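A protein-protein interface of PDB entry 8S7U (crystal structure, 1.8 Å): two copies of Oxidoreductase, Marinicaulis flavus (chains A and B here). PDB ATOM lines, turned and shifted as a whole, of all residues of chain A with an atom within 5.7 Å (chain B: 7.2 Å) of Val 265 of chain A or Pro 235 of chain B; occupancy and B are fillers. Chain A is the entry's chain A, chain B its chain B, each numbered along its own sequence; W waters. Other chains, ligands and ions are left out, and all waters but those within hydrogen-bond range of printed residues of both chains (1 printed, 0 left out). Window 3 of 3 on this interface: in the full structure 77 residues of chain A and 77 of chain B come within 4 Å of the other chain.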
ATOM      1  N   LEU A 260       2.751 -20.881 -35.331  1.00  0.00           N
ATOM      2  CA  LEU A 260       2.700 -19.695 -34.433  1.00  0.00           C
ATOM      3  C   LEU A 260       3.588 -19.916 -33.215  1.00  0.00           C
ATOM      4  O   LEU A 260       4.157 -18.925 -32.709  1.00  0.00           O
ATOM      5  CB  LEU A 260       1.261 -19.427 -33.997  1.00  0.00           C
ATOM      6  CG  LEU A 260       0.327 -18.872 -35.076  1.00  0.00           C
ATOM      7  CD1 LEU A 260      -1.109 -19.037 -34.625  1.00  0.00           C
ATOM      8  CD2 LEU A 260       0.670 -17.446 -35.433  1.00  0.00           C
ATOM      9  N   ARG A 261       3.619 -21.146 -32.681  1.00  0.00           N
ATOM     10  CA  ARG A 261       4.304 -21.424 -31.398  1.00  0.00           C
ATOM     11  C   ARG A 261       5.707 -20.809 -31.373  1.00  0.00           C
ATOM     12  O   ARG A 261       5.991 -19.990 -30.503  1.00  0.00           O
ATOM     13  CB  ARG A 261       4.301 -22.916 -31.107  1.00  0.00           C
ATOM     14  CG  ARG A 261       4.958 -23.236 -29.774  1.00  0.00           C
ATOM     15  CD  ARG A 261       4.952 -24.700 -29.417  1.00  0.00           C
ATOM     16  NE  ARG A 261       5.517 -25.533 -30.478  1.00  0.00           N
ATOM     17  CZ  ARG A 261       4.794 -26.331 -31.253  1.00  0.00           C
ATOM     18  NH1 ARG A 261       3.468 -26.391 -31.122  1.00  0.00           N
ATOM     19  NH2 ARG A 261       5.398 -27.045 -32.188  1.00  0.00           N
ATOM     20  N   PRO A 262       6.696 -21.209 -32.205  1.00  0.00           N
ATOM     21  CA  PRO A 262       8.049 -20.684 -32.044  1.00  0.00           C
ATOM     22  C   PRO A 262       8.127 -19.160 -32.277  1.00  0.00           C
ATOM     23  O   PRO A 262       8.920 -18.512 -31.608  1.00  0.00           O
ATOM     24  CB  PRO A 262       8.896 -21.421 -33.109  1.00  0.00           C
ATOM     25  CG  PRO A 262       7.841 -21.890 -34.125  1.00  0.00           C
ATOM     26  CD  PRO A 262       6.609 -22.205 -33.295  1.00  0.00           C
ATOM     27  N   LEU A 263       7.292 -18.619 -33.170  1.00  0.00           N
ATOM     28  CA  LEU A 263       7.219 -17.146 -33.393  1.00  0.00           C
ATOM     29  C   LEU A 263       6.784 -16.422 -32.101  1.00  0.00           C
ATOM     30  O   LEU A 263       7.358 -15.383 -31.781  1.00  0.00           O
ATOM     31  CB  LEU A 263       6.239 -16.864 -34.525  1.00  0.00           C
ATOM     32  CG  LEU A 263       6.669 -17.343 -35.909  1.00  0.00           C
ATOM     33  CD1 LEU A 263       5.500 -17.217 -36.867  1.00  0.00           C
ATOM     34  CD2 LEU A 263       7.879 -16.580 -36.421  1.00  0.00           C
ATOM     35  N   LYS A 264       5.822 -16.968 -31.381  1.00  0.00           N
ATOM     36  CA  LYS A 264       5.342 -16.335 -30.142  1.00  0.00           C
ATOM     37  C   LYS A 264       6.312 -16.566 -28.996  1.00  0.00           C
ATOM     38  O   LYS A 264       6.692 -15.573 -28.351  1.00  0.00           O
ATOM     39  CB  LYS A 264       3.952 -16.829 -29.776  1.00  0.00           C
ATOM     40  CG  LYS A 264       3.406 -16.103 -28.550  1.00  0.00           C
ATOM     41  CD  LYS A 264       3.162 -14.618 -28.910  1.00  0.00           C
ATOM     42  CE  LYS A 264       2.872 -13.771 -27.714  1.00  0.00           C
ATOM     43  NZ  LYS A 264       2.978 -12.337 -28.051  1.00  0.00           N
ATOM     44  N   VAL A 265       6.835 -17.783 -28.812  1.00  0.00           N
ATOM     45  CA  VAL A 265       7.712 -18.057 -27.644  1.00  0.00           C
ATOM     46  C   VAL A 265       8.989 -17.188 -27.747  1.00  0.00           C
ATOM     47  O   VAL A 265       9.540 -16.784 -26.677  1.00  0.00           O
ATOM     48  CB  VAL A 265       7.987 -19.572 -27.544  1.00  0.00           C
ATOM     49  CG1 VAL A 265       9.022 -19.896 -26.495  1.00  0.00           C
ATOM     50  CG2 VAL A 265       6.725 -20.377 -27.282  1.00  0.00           C
ATOM     51  N   ALA A 266       9.468 -16.864 -28.966  1.00  0.00           N
ATOM     52  CA  ALA A 266      10.674 -16.054 -29.190  1.00  0.00           C
ATOM     53  C   ALA A 266      10.303 -14.578 -29.220  1.00  0.00           C
ATOM     54  O   ALA A 266      11.197 -13.790 -29.215  1.00  0.00           O
ATOM     55  CB  ALA A 266      11.410 -16.432 -30.448  1.00  0.00           C
ATOM     56  N   GLY A 267       9.024 -14.213 -29.190  1.00  0.00           N
ATOM     57  CA  GLY A 267       8.648 -12.779 -29.196  1.00  0.00           C
ATOM     58  C   GLY A 267       8.720 -12.153 -30.586  1.00  0.00           C
ATOM     59  O   GLY A 267       8.518 -10.916 -30.697  1.00  0.00           O
ATOM     60  N   ILE A 396      -0.180 -23.772 -27.213  1.00  0.00           N
ATOM     61  CA  ILE A 396      -0.013 -23.331 -28.628  1.00  0.00           C
ATOM     62  C   ILE A 396       0.457 -24.565 -29.411  1.00  0.00           C
ATOM     63  O   ILE A 396       1.635 -24.643 -29.757  1.00  0.00           O
ATOM     64  CB  ILE A 396       0.914 -22.109 -28.765  1.00  0.00           C
ATOM     65  CG1 ILE A 396       0.628 -21.044 -27.705  1.00  0.00           C
ATOM     66  CG2 ILE A 396       0.831 -21.541 -30.172  1.00  0.00           C
ATOM     67  CD1 ILE A 396       1.560 -19.860 -27.774  1.00  0.00           C
ATOM     68  N   TRP A 427       1.607 -15.531 -24.055  1.00  0.00           N
ATOM     69  CA  TRP A 427       3.063 -15.801 -24.084  1.00  0.00           C
ATOM     70  C   TRP A 427       3.354 -17.268 -24.421  1.00  0.00           C
ATOM     71  O   TRP A 427       4.227 -17.500 -25.245  1.00  0.00           O
ATOM     72  CB  TRP A 427       3.668 -15.379 -22.746  1.00  0.00           C
ATOM     73  CG  TRP A 427       3.731 -13.892 -22.597  1.00  0.00           C
ATOM     74  CD1 TRP A 427       4.309 -13.005 -23.457  1.00  0.00           C
ATOM     75  CD2 TRP A 427       3.185 -13.109 -21.523  1.00  0.00           C
ATOM     76  NE1 TRP A 427       4.168 -11.727 -22.991  1.00  0.00           N
ATOM     77  CE2 TRP A 427       3.482 -11.760 -21.805  1.00  0.00           C
ATOM     78  CE3 TRP A 427       2.482 -13.416 -20.357  1.00  0.00           C
ATOM     79  CZ2 TRP A 427       3.102 -10.721 -20.960  1.00  0.00           C
ATOM     80  CZ3 TRP A 427       2.112 -12.392 -19.521  1.00  0.00           C
ATOM     81  CH2 TRP A 427       2.416 -11.065 -19.820  1.00  0.00           C
ATOM     82  N   ARG A 428       2.625 -18.205 -23.813  1.00  0.00           N
ATOM     83  CA  ARG A 428       2.894 -19.656 -24.029  1.00  0.00           C
ATOM     84  C   ARG A 428       1.570 -20.411 -24.179  1.00  0.00           C
ATOM     85  O   ARG A 428       1.587 -21.636 -24.163  1.00  0.00           O
ATOM     86  CB  ARG A 428       3.737 -20.214 -22.878  1.00  0.00           C
ATOM     87  CG  ARG A 428       5.199 -20.430 -23.232  1.00  0.00           C
ATOM     88  CD  ARG A 428       6.089 -19.375 -22.614  1.00  0.00           C
ATOM     89  NE  ARG A 428       7.498 -19.635 -22.850  1.00  0.00           N
ATOM     90  CZ  ARG A 428       8.436 -18.698 -22.853  1.00  0.00           C
ATOM     91  NH1 ARG A 428       8.102 -17.435 -23.035  1.00  0.00           N
ATOM     92  NH2 ARG A 428       9.702 -19.027 -22.674  1.00  0.00           N
ATOM     93  N   ASN B 116      11.246 -28.313 -21.647  1.00  0.00           N
ATOM     94  CA  ASN B 116      10.476 -28.321 -22.897  1.00  0.00           C
ATOM     95  C   ASN B 116      11.054 -27.262 -23.840  1.00  0.00           C
ATOM     96  O   ASN B 116      10.880 -26.057 -23.566  1.00  0.00           O
ATOM     97  CB  ASN B 116       9.013 -28.067 -22.564  1.00  0.00           C
ATOM     98  CG  ASN B 116       8.119 -28.326 -23.746  1.00  0.00           C
ATOM     99  OD1 ASN B 116       8.227 -27.703 -24.781  1.00  0.00           O
ATOM    100  ND2 ASN B 116       7.181 -29.226 -23.568  1.00  0.00           N
ATOM    101  N   GLU B 117      11.703 -27.683 -24.926  1.00  0.00           N
ATOM    102  CA  GLU B 117      12.284 -26.757 -25.937  1.00  0.00           C
ATOM    103  C   GLU B 117      11.157 -26.048 -26.706  1.00  0.00           C
ATOM    104  O   GLU B 117      11.274 -24.845 -26.931  1.00  0.00           O
ATOM    105  CB  GLU B 117      13.154 -27.515 -26.960  1.00  0.00           C
ATOM    106  CG  GLU B 117      13.944 -26.613 -27.880  1.00  0.00           C
ATOM    107  CD  GLU B 117      14.861 -27.418 -28.810  1.00  0.00           C
ATOM    108  OE1 GLU B 117      14.400 -27.886 -29.830  1.00  0.00           O
ATOM    109  OE2 GLU B 117      16.007 -27.599 -28.481  1.00  0.00           O
ATOM    110  N   GLU B 118      10.116 -26.769 -27.113  1.00  0.00           N
ATOM    111  CA  GLU B 118       9.080 -26.221 -28.016  1.00  0.00           C
ATOM    112  C   GLU B 118       8.385 -25.039 -27.294  1.00  0.00           C
ATOM    113  O   GLU B 118       8.044 -24.030 -27.941  1.00  0.00           O
ATOM    114  CB  GLU B 118       8.056 -27.306 -28.322  1.00  0.00           C
ATOM    115  CG  GLU B 118       8.608 -28.420 -29.187  1.00  0.00           C
ATOM    116  CD  GLU B 118       9.502 -29.477 -28.506  1.00  0.00           C
ATOM    117  OE1 GLU B 118       9.504 -29.647 -27.212  1.00  0.00           O
ATOM    118  OE2 GLU B 118      10.249 -30.155 -29.279  1.00  0.00           O
ATOM    119  N   PHE B 119       8.150 -25.158 -25.992  1.00  0.00           N
ATOM    120  CA  PHE B 119       7.446 -24.100 -25.210  1.00  0.00           C
ATOM    121  C   PHE B 119       8.394 -23.300 -24.333  1.00  0.00           C
ATOM    122  O   PHE B 119       7.934 -22.364 -23.661  1.00  0.00           O
ATOM    123  CB  PHE B 119       6.346 -24.696 -24.364  1.00  0.00           C
ATOM    124  CG  PHE B 119       5.111 -24.987 -25.161  1.00  0.00           C
ATOM    125  CD1 PHE B 119       4.334 -23.920 -25.633  1.00  0.00           C
ATOM    126  CD2 PHE B 119       4.751 -26.278 -25.451  1.00  0.00           C
ATOM    127  CE1 PHE B 119       3.156 -24.166 -26.320  1.00  0.00           C
ATOM    128  CE2 PHE B 119       3.621 -26.534 -26.218  1.00  0.00           C
ATOM    129  CZ  PHE B 119       2.848 -25.480 -26.663  1.00  0.00           C
ATOM    130  N   GLY B 120       9.679 -23.629 -24.324  1.00  0.00           N
ATOM    131  CA  GLY B 120      10.638 -22.869 -23.520  1.00  0.00           C
ATOM    132  C   GLY B 120      10.253 -22.809 -22.062  1.00  0.00           C
ATOM    133  O   GLY B 120       9.928 -21.733 -21.575  1.00  0.00           O
ATOM    134  N   TYR B 121      10.319 -23.926 -21.331  1.00  0.00           N
ATOM    135  CA  TYR B 121      10.136 -23.929 -19.861  1.00  0.00           C
ATOM    136  C   TYR B 121      10.881 -25.114 -19.255  1.00  0.00           C
ATOM    137  O   TYR B 121      11.227 -26.093 -19.958  1.00  0.00           O
ATOM    138  CB  TYR B 121       8.655 -23.977 -19.511  1.00  0.00           C
ATOM    139  CG  TYR B 121       7.907 -25.252 -19.777  1.00  0.00           C
ATOM    140  CD1 TYR B 121       8.066 -26.366 -18.962  1.00  0.00           C
ATOM    141  CD2 TYR B 121       6.980 -25.355 -20.796  1.00  0.00           C
ATOM    142  CE1 TYR B 121       7.346 -27.529 -19.182  1.00  0.00           C
ATOM    143  CE2 TYR B 121       6.233 -26.507 -21.010  1.00  0.00           C
ATOM    144  CZ  TYR B 121       6.432 -27.606 -20.194  1.00  0.00           C
ATOM    145  OH  TYR B 121       5.717 -28.745 -20.401  1.00  0.00           O
ATOM    146  N   LYS B 143      17.864 -25.950 -27.339  1.00  0.00           N
ATOM    147  CA  LYS B 143      18.202 -24.574 -27.794  1.00  0.00           C
ATOM    148  C   LYS B 143      17.524 -23.546 -26.850  1.00  0.00           C
ATOM    149  O   LYS B 143      16.647 -22.818 -27.289  1.00  0.00           O
ATOM    150  CB  LYS B 143      17.652 -24.431 -29.213  1.00  0.00           C
ATOM    151  CG  LYS B 143      18.149 -25.494 -30.191  1.00  0.00           C
ATOM    152  CD  LYS B 143      19.625 -25.793 -30.041  1.00  0.00           C
ATOM    153  CE  LYS B 143      20.072 -26.931 -30.953  1.00  0.00           C
ATOM    154  NZ  LYS B 143      21.540 -26.920 -31.059  1.00  0.00           N
ATOM    155  N   LEU B 144      17.879 -23.586 -25.576  1.00  0.00           N
ATOM    156  CA  LEU B 144      17.320 -22.723 -24.508  1.00  0.00           C
ATOM    157  C   LEU B 144      18.467 -22.143 -23.737  1.00  0.00           C
ATOM    158  O   LEU B 144      19.489 -22.861 -23.520  1.00  0.00           O
ATOM    159  CB  LEU B 144      16.489 -23.575 -23.550  1.00  0.00           C
ATOM    160  CG  LEU B 144      15.287 -24.237 -24.184  1.00  0.00           C
ATOM    161  CD1 LEU B 144      14.646 -25.212 -23.223  1.00  0.00           C
ATOM    162  CD2 LEU B 144      14.314 -23.208 -24.673  1.00  0.00           C
ATOM    163  N   TRP B 145      18.240 -20.948 -23.213  1.00  0.00           N
ATOM    164  CA  TRP B 145      19.135 -20.318 -22.230  1.00  0.00           C
ATOM    165  C   TRP B 145      18.433 -20.268 -20.887  1.00  0.00           C
ATOM    166  O   TRP B 145      17.218 -20.186 -20.847  1.00  0.00           O
ATOM    167  CB  TRP B 145      19.553 -18.915 -22.707  1.00  0.00           C
ATOM    168  CG  TRP B 145      20.462 -18.920 -23.880  1.00  0.00           C
ATOM    169  CD1 TRP B 145      21.032 -20.015 -24.460  1.00  0.00           C
ATOM    170  CD2 TRP B 145      21.087 -17.772 -24.482  1.00  0.00           C
ATOM    171  NE1 TRP B 145      21.865 -19.616 -25.461  1.00  0.00           N
ATOM    172  CE2 TRP B 145      21.950 -18.256 -25.472  1.00  0.00           C
ATOM    173  CE3 TRP B 145      20.978 -16.392 -24.309  1.00  0.00           C
ATOM    174  CZ2 TRP B 145      22.660 -17.395 -26.311  1.00  0.00           C
ATOM    175  CZ3 TRP B 145      21.695 -15.542 -25.112  1.00  0.00           C
ATOM    176  CH2 TRP B 145      22.519 -16.043 -26.100  1.00  0.00           C
ATOM    177  N   TYR B 170      15.336 -12.501 -19.300  1.00  0.00           N
ATOM    178  CA  TYR B 170      14.540 -13.269 -18.306  1.00  0.00           C
ATOM    179  C   TYR B 170      15.086 -12.990 -16.891  1.00  0.00           C
ATOM    180  O   TYR B 170      14.887 -13.830 -16.021  1.00  0.00           O
ATOM    181  CB  TYR B 170      14.539 -14.739 -18.723  1.00  0.00           C
ATOM    182  CG  TYR B 170      13.579 -15.130 -19.820  1.00  0.00           C
ATOM    183  CD1 TYR B 170      13.530 -14.450 -21.024  1.00  0.00           C
ATOM    184  CD2 TYR B 170      12.733 -16.211 -19.661  1.00  0.00           C
ATOM    185  CE1 TYR B 170      12.649 -14.815 -22.027  1.00  0.00           C
ATOM    186  CE2 TYR B 170      11.842 -16.586 -20.649  1.00  0.00           C
ATOM    187  CZ  TYR B 170      11.806 -15.894 -21.841  1.00  0.00           C
ATOM    188  OH  TYR B 170      10.941 -16.285 -22.817  1.00  0.00           O
ATOM    189  N   LEU B 233      11.805 -20.251 -19.984  1.00  0.00           N
ATOM    190  CA  LEU B 233      13.201 -20.172 -20.411  1.00  0.00           C
ATOM    191  C   LEU B 233      13.245 -19.525 -21.796  1.00  0.00           C
ATOM    192  O   LEU B 233      12.382 -19.805 -22.623  1.00  0.00           O
ATOM    193  CB  LEU B 233      13.803 -21.583 -20.519  1.00  0.00           C
ATOM    194  CG  LEU B 233      13.963 -22.371 -19.237  1.00  0.00           C
ATOM    195  CD1 LEU B 233      14.539 -23.749 -19.605  1.00  0.00           C
ATOM    196  CD2 LEU B 233      14.842 -21.640 -18.211  1.00  0.00           C
ATOM    197  N   MET B 234      14.245 -18.705 -22.024  1.00  0.00           N
ATOM    198  CA  MET B 234      14.389 -17.997 -23.304  1.00  0.00           C
ATOM    199  C   MET B 234      14.898 -18.967 -24.386  1.00  0.00           C
ATOM    200  O   MET B 234      15.952 -19.627 -24.224  1.00  0.00           O
ATOM    201  CB  MET B 234      15.408 -16.881 -23.147  1.00  0.00           C
ATOM    202  CG  MET B 234      15.473 -15.988 -24.378  1.00  0.00           C
ATOM    203  SD  MET B 234      16.453 -14.521 -23.978  1.00  0.00           S
ATOM    204  CE  MET B 234      18.100 -15.134 -23.997  1.00  0.00           C
ATOM    205  N   PRO B 235      14.247 -18.990 -25.555  1.00  0.00           N
ATOM    206  CA  PRO B 235      14.821 -19.666 -26.725  1.00  0.00           C
ATOM    207  C   PRO B 235      16.168 -19.036 -27.095  1.00  0.00           C
ATOM    208  O   PRO B 235      16.342 -17.817 -27.040  1.00  0.00           O
ATOM    209  CB  PRO B 235      13.761 -19.484 -27.823  1.00  0.00           C
ATOM    210  CG  PRO B 235      12.505 -19.087 -27.105  1.00  0.00           C
ATOM    211  CD  PRO B 235      12.964 -18.359 -25.853  1.00  0.00           C
ATOM    212  N   GLU B 236      17.128 -19.881 -27.520  1.00  0.00           N
ATOM    213  CA  GLU B 236      18.427 -19.389 -27.984  1.00  0.00           C
ATOM    214  C   GLU B 236      18.122 -18.365 -29.070  1.00  0.00           C
ATOM    215  O   GLU B 236      17.365 -18.644 -29.996  1.00  0.00           O
ATOM    216  CB  GLU B 236      19.281 -20.550 -28.532  1.00  0.00           C
ATOM    217  CG  GLU B 236      20.571 -20.093 -29.095  1.00  0.00           C
ATOM    218  CD  GLU B 236      21.488 -21.286 -29.339  1.00  0.00           C
ATOM    219  OE1 GLU B 236      21.006 -22.218 -30.008  1.00  0.00           O
ATOM    220  OE2 GLU B 236      22.623 -21.285 -28.779  1.00  0.00           O
ATOM    221  N   PRO B 237      18.655 -17.154 -28.968  1.00  0.00           N
ATOM    222  CA  PRO B 237      18.355 -16.109 -29.948  1.00  0.00           C
ATOM    223  C   PRO B 237      19.209 -16.235 -31.216  1.00  0.00           C
ATOM    224  O   PRO B 237      20.122 -17.031 -31.254  1.00  0.00           O
ATOM    225  CB  PRO B 237      18.696 -14.821 -29.201  1.00  0.00           C
ATOM    226  CG  PRO B 237      19.775 -15.226 -28.275  1.00  0.00           C
ATOM    227  CD  PRO B 237      19.469 -16.663 -27.866  1.00  0.00           C
ATOM    228  N   ALA B 238      18.876 -15.460 -32.237  1.00  0.00           N
ATOM    229  CA  ALA B 238      19.529 -15.543 -33.564  1.00  0.00           C
ATOM    230  C   ALA B 238      20.848 -14.774 -33.537  1.00  0.00           C
ATOM    231  O   ALA B 238      21.552 -14.828 -34.518  1.00  0.00           O
ATOM    232  CB  ALA B 238      18.606 -14.970 -34.614  1.00  0.00           C
HETATM  233  O   HOH W   1      11.159 -15.216 -25.272  1.00  0.00           O
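NE of Arg 428 of chain A lies within hydrogen-bond range of O of Phe 119 of chain B (2.9 Å). The backbone carbonyl oxygen (O) of Gly 120 of chain B lies within hydrogen-bond range of the guanidinium group (NH2) of Arg 428 of chain A (2.9 Å). The guanidinium group of Arg 428 of chain A lies within hydrogen-bond range of the side-chain hydroxyl of Tyr 170 of chain B. The guanidinium group of Arg 428 of chain A is in hydrogen-bond range of the backbone carbonyl oxygen of Leu 233 of chain B (2.8 Å).
NH1 of Arg 261 of chain A lies within hydrogen-bond range of O of Ile 396 of chain A (2.9 Å). N of Glu 118 of chain B lies within hydrogen-bond range of OD1 of Asn 116 of chain B, at 3.1 Å. The backbone NH (N) of Phe 119 of chain B is in hydrogen-bond range of the side-chain amide oxygen (OD1) of Asn 116 of chain B (2.8 Å). O of Gly 120 of chain B is in hydrogen-bond range of N of Leu 233 of chain B (2.9 Å).
Among the printed residues, pairs that only touch across the chains: Ile 396 of chain A with Phe 119 of chain B (3.4 Å), Arg 261 of chain A with Glu 118 of chain B (3.5 Å), Arg 261 of chain A with Phe 119 of chain B (3.6 Å), Val 265 of chain A with Pro 235 of chain B (3.6 Å), Val 265 of chain A with Phe 119 of chain B (3.9 Å) and Val 265 of chain A with Glu 118 of chain B (3.9 Å).
Of chain B, only Glu 118 (3.9 Å), Phe 119 (3.9 Å) and Pro 235 (3.6 Å) come within 4 Å of Val 265 of chain A. Pro 235 of chain B touches just one residue of chain A: Val 265 (3.6 Å). Printed residues of chain A within 4 Å of Glu 118 of chain B: Arg 261 and Val 265. Printed residues of chain A within 4 Å of Gly 120 of chain B: Arg 428 (2.9 Å). Printed residues of chain A within 4 Å of Tyr 170 of chain B: Arg 428 (3.0 Å). Of the printed residues of chain B, Ile 396 of chain A touches Phe 119. Of the printed residues of chain A, Leu 233 of chain B touches Arg 428. Gly 267 of chain A touches none of the printed residues of chain B. The nearest residue of chain B that does not touch Val 265 of chain A is Tyr 170 of chain B (4.1 Å). The nearest printed residue of chain A that does not touch Leu 233 of chain B is Val 265 of chain A (5.1 Å).
Printed residues of chain A that touch a printed residue of chain B: Arg 261, Val 265, Ile 396 and Arg 428. Hydrophobic or aromatic side chains of chain A within 4 Å of the printed part of chain B: Val 265 and Ile 396. Of the 16 printed residues of chain B, 6 touch a printed residue of chain A. Printed residues of chain B that touch a printed residue of chain A: Glu 118, Phe 119, Gly 120, Tyr 170, Leu 233 and Pro 235. Along chain B the printed residues that touch a printed residue of chain A span positions 118 to 235. Among the printed residues, 10 pairs touch across the chains. Among the printed residues, no Asp or Glu carboxylate lies within 4 Å of a Lys or Arg side-chain nitrogen of the other chain.
No position is printed for both chains.
Water W1 lies within hydrogen-bond range of O of Val 265 of chain A (2.7 Å) and OH of Tyr 170 of chain B (2.7 Å).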
